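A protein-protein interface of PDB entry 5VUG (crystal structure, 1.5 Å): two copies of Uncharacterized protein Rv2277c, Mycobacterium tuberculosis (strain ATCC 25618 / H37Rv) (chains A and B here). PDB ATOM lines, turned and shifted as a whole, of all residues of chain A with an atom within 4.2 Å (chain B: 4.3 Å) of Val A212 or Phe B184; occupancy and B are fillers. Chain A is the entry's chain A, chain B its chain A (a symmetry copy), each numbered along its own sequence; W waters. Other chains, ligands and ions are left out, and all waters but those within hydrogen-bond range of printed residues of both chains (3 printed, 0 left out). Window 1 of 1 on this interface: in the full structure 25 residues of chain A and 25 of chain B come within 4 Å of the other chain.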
ATOM      1  N   LEU A 188     -29.829  12.230 -25.115  1.00  0.00           N
ATOM      2  CA  LEU A 188     -28.493  12.047 -25.662  1.00  0.00           C
ATOM      3  C   LEU A 188     -28.411  11.019 -26.783  1.00  0.00           C
ATOM      4  O   LEU A 188     -27.485  11.098 -27.597  1.00  0.00           O
ATOM      5  CB  LEU A 188     -27.480  11.717 -24.550  1.00  0.00           C
ATOM      6  CG  LEU A 188     -27.258  12.825 -23.517  1.00  0.00           C
ATOM      7  CD1 LEU A 188     -26.375  12.331 -22.377  1.00  0.00           C
ATOM      8  CD2 LEU A 188     -26.633  14.045 -24.183  1.00  0.00           C
ATOM      9  N   THR A 211     -23.083  17.306 -14.255  1.00  0.00           N
ATOM     10  CA  THR A 211     -21.748  17.216 -14.825  1.00  0.00           C
ATOM     11  C   THR A 211     -21.683  15.984 -15.707  1.00  0.00           C
ATOM     12  O   THR A 211     -22.231  14.933 -15.365  1.00  0.00           O
ATOM     13  CB  THR A 211     -20.638  17.149 -13.769  1.00  0.00           C
ATOM     14  OG1 THR A 211     -20.676  15.877 -13.113  1.00  0.00           O
ATOM     15  CG2 THR A 211     -20.796  18.254 -12.757  1.00  0.00           C
ATOM     16  N   VAL A 212     -21.028  16.129 -16.851  1.00  0.00           N
ATOM     17  CA  VAL A 212     -20.832  15.040 -17.797  1.00  0.00           C
ATOM     18  C   VAL A 212     -19.352  14.707 -17.806  1.00  0.00           C
ATOM     19  O   VAL A 212     -18.518  15.602 -17.982  1.00  0.00           O
ATOM     20  CB  VAL A 212     -21.300  15.454 -19.202  1.00  0.00           C
ATOM     21  CG1 VAL A 212     -20.960  14.369 -20.195  1.00  0.00           C
ATOM     22  CG2 VAL A 212     -22.800  15.733 -19.194  1.00  0.00           C
ATOM     23  N   THR A 213     -19.022  13.429 -17.628  1.00  0.00           N
ATOM     24  CA  THR A 213     -17.635  12.987 -17.573  1.00  0.00           C
ATOM     25  C   THR A 213     -17.385  11.932 -18.642  1.00  0.00           C
ATOM     26  O   THR A 213     -18.154  10.976 -18.763  1.00  0.00           O
ATOM     27  CB  THR A 213     -17.305  12.395 -16.200  1.00  0.00           C
ATOM     28  OG1 THR A 213     -17.645  13.333 -15.174  1.00  0.00           O
ATOM     29  CG2 THR A 213     -15.820  12.072 -16.109  1.00  0.00           C
ATOM     30  N   GLY A 221     -12.297  13.934 -18.972  1.00  0.00           N
ATOM     31  CA  GLY A 221     -12.781  15.254 -19.341  1.00  0.00           C
ATOM     32  C   GLY A 221     -14.157  15.469 -18.750  1.00  0.00           C
ATOM     33  O   GLY A 221     -14.997  14.574 -18.772  1.00  0.00           O
ATOM     34  N   ILE A 222     -14.378  16.670 -18.214  1.00  0.00           N
ATOM     35  CA  ILE A 222     -15.605  16.992 -17.492  1.00  0.00           C
ATOM     36  C   ILE A 222     -16.208  18.272 -18.057  1.00  0.00           C
ATOM     37  O   ILE A 222     -15.489  19.241 -18.332  1.00  0.00           O
ATOM     38  CB  ILE A 222     -15.355  17.148 -15.974  1.00  0.00           C
ATOM     39  CG1 ILE A 222     -14.640  15.921 -15.404  1.00  0.00           C
ATOM     40  CG2 ILE A 222     -16.676  17.365 -15.238  1.00  0.00           C
ATOM     41  CD1 ILE A 222     -13.912  16.187 -14.090  1.00  0.00           C
ATOM     42  N   SER A 223     -17.531  18.281 -18.213  1.00  0.00           N
ATOM     43  CA  SER A 223     -18.268  19.475 -18.609  1.00  0.00           C
ATOM     44  C   SER A 223     -19.432  19.690 -17.658  1.00  0.00           C
ATOM     45  O   SER A 223     -20.199  18.760 -17.387  1.00  0.00           O
ATOM     46  CB  SER A 223     -18.804  19.350 -20.038  1.00  0.00           C
ATOM     47  OG  SER A 223     -17.741  19.161 -20.954  1.00  0.00           O
ATOM     48  N   VAL A 225     -23.015  21.272 -17.333  1.00  0.00           N
ATOM     49  CA  VAL A 225     -24.050  21.559 -18.323  1.00  0.00           C
ATOM     50  C   VAL A 225     -25.390  21.651 -17.616  1.00  0.00           C
ATOM     51  O   VAL A 225     -25.687  20.851 -16.723  1.00  0.00           O
ATOM     52  CB  VAL A 225     -24.132  20.459 -19.408  1.00  0.00           C
ATOM     53  CG1 VAL A 225     -25.067  20.885 -20.554  1.00  0.00           C
ATOM     54  CG2 VAL A 225     -22.751  20.108 -19.947  1.00  0.00           C
ATOM     55  N   ARG B 180     -16.489  19.610 -26.554  1.00  0.00           N
ATOM     56  CA  ARG B 180     -17.411  18.805 -25.753  1.00  0.00           C
ATOM     57  C   ARG B 180     -18.470  19.670 -25.080  1.00  0.00           C
ATOM     58  O   ARG B 180     -19.645  19.286 -25.014  1.00  0.00           O
ATOM     59  CB  ARG B 180     -16.639  18.005 -24.697  1.00  0.00           C
ATOM     60  CG  ARG B 180     -17.501  16.995 -23.919  1.00  0.00           C
ATOM     61  CD  ARG B 180     -16.711  16.243 -22.832  1.00  0.00           C
ATOM     62  NE  ARG B 180     -16.034  17.195 -21.956  1.00  0.00           N
ATOM     63  CZ  ARG B 180     -14.717  17.384 -21.913  1.00  0.00           C
ATOM     64  NH1 ARG B 180     -13.899  16.640 -22.656  1.00  0.00           N
ATOM     65  NH2 ARG B 180     -14.216  18.318 -21.118  1.00  0.00           N
ATOM     66  N   GLN B 181     -18.068  20.830 -24.554  1.00  0.00           N
ATOM     67  CA  GLN B 181     -19.020  21.737 -23.920  1.00  0.00           C
ATOM     68  C   GLN B 181     -20.088  22.191 -24.910  1.00  0.00           C
ATOM     69  O   GLN B 181     -21.283  22.194 -24.595  1.00  0.00           O
ATOM     70  CB  GLN B 181     -18.275  22.947 -23.369  1.00  0.00           C
ATOM     71  CG  GLN B 181     -19.178  23.908 -22.628  1.00  0.00           C
ATOM     72  CD  GLN B 181     -19.599  23.355 -21.289  1.00  0.00           C
ATOM     73  OE1 GLN B 181     -18.763  23.111 -20.415  1.00  0.00           O
ATOM     74  NE2 GLN B 181     -20.893  23.132 -21.122  1.00  0.00           N
ATOM     75  N   ARG B 182     -19.671  22.576 -26.121  1.00  0.00           N
ATOM     76  CA  ARG B 182     -20.636  23.048 -27.106  1.00  0.00           C
ATOM     77  C   ARG B 182     -21.581  21.927 -27.523  1.00  0.00           C
ATOM     78  O   ARG B 182     -22.793  22.146 -27.648  1.00  0.00           O
ATOM     79  CB  ARG B 182     -19.918  23.645 -28.319  1.00  0.00           C
ATOM     80  CG  ARG B 182     -20.825  24.550 -29.137  1.00  0.00           C
ATOM     81  CD  ARG B 182     -20.159  25.147 -30.375  1.00  0.00           C
ATOM     82  NE  ARG B 182     -19.026  26.025 -30.079  1.00  0.00           N
ATOM     83  CZ  ARG B 182     -17.751  25.667 -30.206  1.00  0.00           C
ATOM     84  NH1 ARG B 182     -17.440  24.440 -30.612  1.00  0.00           N
ATOM     85  NH2 ARG B 182     -16.789  26.530 -29.926  1.00  0.00           N
ATOM     86  N   LEU B 183     -21.051  20.715 -27.714  1.00  0.00           N
ATOM     87  CA  LEU B 183     -21.894  19.592 -28.115  1.00  0.00           C
ATOM     88  C   LEU B 183     -22.899  19.241 -27.031  1.00  0.00           C
ATOM     89  O   LEU B 183     -24.064  18.952 -27.329  1.00  0.00           O
ATOM     90  CB  LEU B 183     -21.033  18.370 -28.419  1.00  0.00           C
ATOM     91  CG  LEU B 183     -20.275  18.412 -29.743  1.00  0.00           C
ATOM     92  CD1 LEU B 183     -19.287  17.258 -29.762  1.00  0.00           C
ATOM     93  CD2 LEU B 183     -21.251  18.353 -30.938  1.00  0.00           C
ATOM     94  N   PHE B 184     -22.465  19.235 -25.768  1.00  0.00           N
ATOM     95  CA  PHE B 184     -23.389  18.889 -24.697  1.00  0.00           C
ATOM     96  C   PHE B 184     -24.389  20.005 -24.420  1.00  0.00           C
ATOM     97  O   PHE B 184     -25.548  19.722 -24.089  1.00  0.00           O
ATOM     98  CB  PHE B 184     -22.643  18.418 -23.446  1.00  0.00           C
ATOM     99  CG  PHE B 184     -22.300  16.952 -23.483  1.00  0.00           C
ATOM    100  CD1 PHE B 184     -23.275  15.996 -23.218  1.00  0.00           C
ATOM    101  CD2 PHE B 184     -21.025  16.523 -23.826  1.00  0.00           C
ATOM    102  CE1 PHE B 184     -22.982  14.640 -23.269  1.00  0.00           C
ATOM    103  CE2 PHE B 184     -20.722  15.160 -23.878  1.00  0.00           C
ATOM    104  CZ  PHE B 184     -21.706  14.222 -23.594  1.00  0.00           C
ATOM    105  N   ASN B 185     -23.986  21.270 -24.557  1.00  0.00           N
ATOM    106  CA  ASN B 185     -24.981  22.339 -24.466  1.00  0.00           C
ATOM    107  C   ASN B 185     -26.041  22.184 -25.551  1.00  0.00           C
ATOM    108  O   ASN B 185     -27.243  22.291 -25.282  1.00  0.00           O
ATOM    109  CB  ASN B 185     -24.317  23.716 -24.548  1.00  0.00           C
ATOM    110  CG  ASN B 185     -23.836  24.223 -23.194  1.00  0.00           C
ATOM    111  OD1 ASN B 185     -24.404  23.885 -22.151  1.00  0.00           O
ATOM    112  ND2 ASN B 185     -22.785  25.046 -23.206  1.00  0.00           N
ATOM    113  N   MET B 186     -25.622  21.915 -26.784  1.00  0.00           N
ATOM    114  CA  MET B 186     -26.622  21.713 -27.829  1.00  0.00           C
ATOM    115  C   MET B 186     -27.560  20.539 -27.526  1.00  0.00           C
ATOM    116  O   MET B 186     -28.784  20.664 -27.655  1.00  0.00           O
ATOM    117  CB  MET B 186     -25.972  21.584 -29.213  1.00  0.00           C
ATOM    118  CG  MET B 186     -25.486  22.907 -29.765  1.00  0.00           C
ATOM    119  SD  MET B 186     -26.987  24.085 -30.195  1.00  0.00           S
ATOM    120  CE  MET B 186     -27.846  22.958 -31.535  1.00  0.00           C
ATOM    121  N   ALA B 187     -26.987  19.415 -27.089  1.00  0.00           N
ATOM    122  CA  ALA B 187     -27.788  18.215 -26.869  1.00  0.00           C
ATOM    123  C   ALA B 187     -28.732  18.379 -25.685  1.00  0.00           C
ATOM    124  O   ALA B 187     -29.852  17.854 -25.700  1.00  0.00           O
ATOM    125  CB  ALA B 187     -26.875  17.008 -26.649  1.00  0.00           C
ATOM    126  N   LEU B 188     -28.301  19.088 -24.644  1.00  0.00           N
ATOM    127  CA  LEU B 188     -29.055  19.093 -23.399  1.00  0.00           C
ATOM    128  C   LEU B 188     -29.886  20.350 -23.177  1.00  0.00           C
ATOM    129  O   LEU B 188     -30.871  20.289 -22.434  1.00  0.00           O
ATOM    130  CB  LEU B 188     -28.134  18.833 -22.193  1.00  0.00           C
ATOM    131  CG  LEU B 188     -27.469  17.455 -22.162  1.00  0.00           C
ATOM    132  CD1 LEU B 188     -26.455  17.369 -21.027  1.00  0.00           C
ATOM    133  CD2 LEU B 188     -28.526  16.366 -22.014  1.00  0.00           C
ATOM    134  N   VAL B 210     -20.528   8.261 -21.601  1.00  0.00           N
ATOM    135  CA  VAL B 210     -20.265   9.288 -20.602  1.00  0.00           C
ATOM    136  C   VAL B 210     -20.993   8.922 -19.317  1.00  0.00           C
ATOM    137  O   VAL B 210     -21.832   8.023 -19.281  1.00  0.00           O
ATOM    138  CB  VAL B 210     -20.665  10.702 -21.077  1.00  0.00           C
ATOM    139  CG1 VAL B 210     -19.853  11.096 -22.302  1.00  0.00           C
ATOM    140  CG2 VAL B 210     -22.154  10.776 -21.367  1.00  0.00           C
ATOM    141  N   THR B 211     -20.649   9.618 -18.242  1.00  0.00           N
ATOM    142  CA  THR B 211     -21.448   9.544 -17.028  1.00  0.00           C
ATOM    143  C   THR B 211     -22.000  10.925 -16.731  1.00  0.00           C
ATOM    144  O   THR B 211     -21.308  11.931 -16.899  1.00  0.00           O
ATOM    145  CB  THR B 211     -20.664   9.033 -15.813  1.00  0.00           C
ATOM    146  OG1 THR B 211     -19.727  10.031 -15.392  1.00  0.00           O
ATOM    147  CG2 THR B 211     -19.938   7.755 -16.145  1.00  0.00           C
ATOM    148  N   VAL B 212     -23.257  10.963 -16.307  1.00  0.00           N
ATOM    149  CA  VAL B 212     -23.931  12.198 -15.936  1.00  0.00           C
ATOM    150  C   VAL B 212     -24.170  12.153 -14.439  1.00  0.00           C
ATOM    151  O   VAL B 212     -24.728  11.173 -13.931  1.00  0.00           O
ATOM    152  CB  VAL B 212     -25.264  12.334 -16.690  1.00  0.00           C
ATOM    153  CG1 VAL B 212     -26.015  13.544 -16.189  1.00  0.00           C
ATOM    154  CG2 VAL B 212     -25.010  12.435 -18.191  1.00  0.00           C
ATOM    155  N   ALA B 227     -23.787   8.859 -25.578  1.00  0.00           N
ATOM    156  CA  ALA B 227     -24.167  10.124 -26.194  1.00  0.00           C
ATOM    157  C   ALA B 227     -23.886  10.095 -27.693  1.00  0.00           C
ATOM    158  O   ALA B 227     -22.780   9.743 -28.118  1.00  0.00           O
ATOM    159  CB  ALA B 227     -23.389  11.273 -25.557  1.00  0.00           C
ATOM    160  N   LEU B 229     -23.811  12.867 -30.297  1.00  0.00           N
ATOM    161  CA  LEU B 229     -23.829  14.322 -30.186  1.00  0.00           C
ATOM    162  C   LEU B 229     -23.872  15.059 -31.516  1.00  0.00           C
ATOM    163  O   LEU B 229     -24.181  16.257 -31.526  1.00  0.00           O
ATOM    164  CB  LEU B 229     -22.610  14.801 -29.395  1.00  0.00           C
ATOM    165  CG  LEU B 229     -22.627  14.324 -27.941  1.00  0.00           C
ATOM    166  CD1 LEU B 229     -21.264  14.572 -27.317  1.00  0.00           C
ATOM    167  CD2 LEU B 229     -23.731  15.021 -27.140  1.00  0.00           C
HETATM  168  O   HOH W   1     -11.829  18.495 -18.843  1.00  0.00           O
HETATM  169  O   HOH W   2     -20.301  12.984 -14.372  1.00  0.00           O
HETATM  170  O   HOH W   3     -15.884  20.943 -21.250  1.00  0.00           O
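Among the printed residues, merely in contact across the chains: Thr A213 with Val B210 (3.3 Å), Thr A211 with Val B212 (3.3 Å), Val A212 with Thr B211 (3.3 Å), Val A225 with Asn B185 (3.5 Å), Val A212 with Phe B184 (3.5 Å), Leu A188 with Leu B188 (3.7 Å), Gly A221 with Arg B180 (3.7 Å), Leu A188 with Ala B227 (3.7 Å), Val A225 with Gln B181 (3.7 Å), Val A225 with Phe B184 (3.8 Å), Ser A223 with Gln B181 (3.8 Å), Val A212 with Val B210 (3.8 Å), Val A225 with Leu B188 (3.8 Å), Leu A188 with Phe B184 (3.8 Å) and Leu A188 with Ala B187 (3.9 Å).
Of chain B, only Phe B184 (3.5 Å), Val B210 (3.8 Å) and Thr B211 (3.3 Å) come within 4 Å of Val A212.
Of chain A, only Leu A188, Val A212 and Val A225 come within 4 Å of Phe B184.
Of the printed residues of chain A, Leu B188 touches Leu A188 and Val A225.
Of the printed residues of chain B, Ser A223 touches Arg B180 and Gln B181.
Of the printed residues of chain A, Gln B181 touches Ser A223 (3.8 Å) and Val A225 (3.7 Å).
The nearest residue of chain B that does not touch Val A212 is Val B212 (4.1 Å).
The nearest printed residue of chain A that does not touch Phe B184 is Ser A223 (5.1 Å).
Water W3 lies within hydrogen-bond range of the side-chain hydroxyl of Ser A223 (2.6 Å), the guanidinium group of Arg B180 (3.1 Å) and the backbone carbonyl oxygen of Ile A222 (3.4 Å).
Water W2 lies within hydrogen-bond range of the side-chain hydroxyl (OG1) of Thr A213, the backbone carbonyl oxygen (O) of Thr A211 and the backbone carbonyl oxygen (O) of Thr B211.
Water W1 bridges the backbone NH (N) of Ile A222 (3.2 Å) and the guanidinium group (NH2) of Arg B180 (3.3 Å).
Leu A188 touches its own counterpart, Leu B188.
Thr B211 touches its own counterpart, Thr A211.
Thr A211 touches Val B212, and with the chains exchanged Val A212 touches Thr B211.
N of Val A212 lies within hydrogen-bond range of O of Ser A223 (2.8 Å).
The side-chain amide nitrogen (NE2) of Gln B181 lies close to the side-chain amide nitrogen (ND2) of Asn B185, 3.4 Å away.
The backbone carbonyl oxygen of Thr B211 sits at hydrogen-bond distance from the backbone NH of Thr A213, 2.8 Å away.
O of Ile A222 sits at hydrogen-bond distance from NH2 of Arg B180 (3.2 Å).
OG of Ser A223 lies within hydrogen-bond range of NE of Arg B180 (2.8 Å).
The backbone carbonyl oxygen of Thr B211 sits close to the backbone carbonyl oxygen of Thr A211, 3.5 Å away.
Of the 8 printed residues of chain A, 8 touch a printed residue of chain B.
Hydrophobic or aromatic side chains of chain A that line the printed part of chain B: Leu A188, Val A212 and Val A225.
Of the 14 printed residues of chain B, 10 touch a printed residue of chain A.
Hydrophobic or aromatic side chains of chain B that line the printed part of chain A: Phe B184, Ala B187, Leu B188 and Val B210.
Among the printed residues, 19 pairs touch across the chains.
Among the printed residues, no Asp or Glu carboxylate lies within 4 Å of a Lys or Arg side-chain nitrogen of the other chain.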
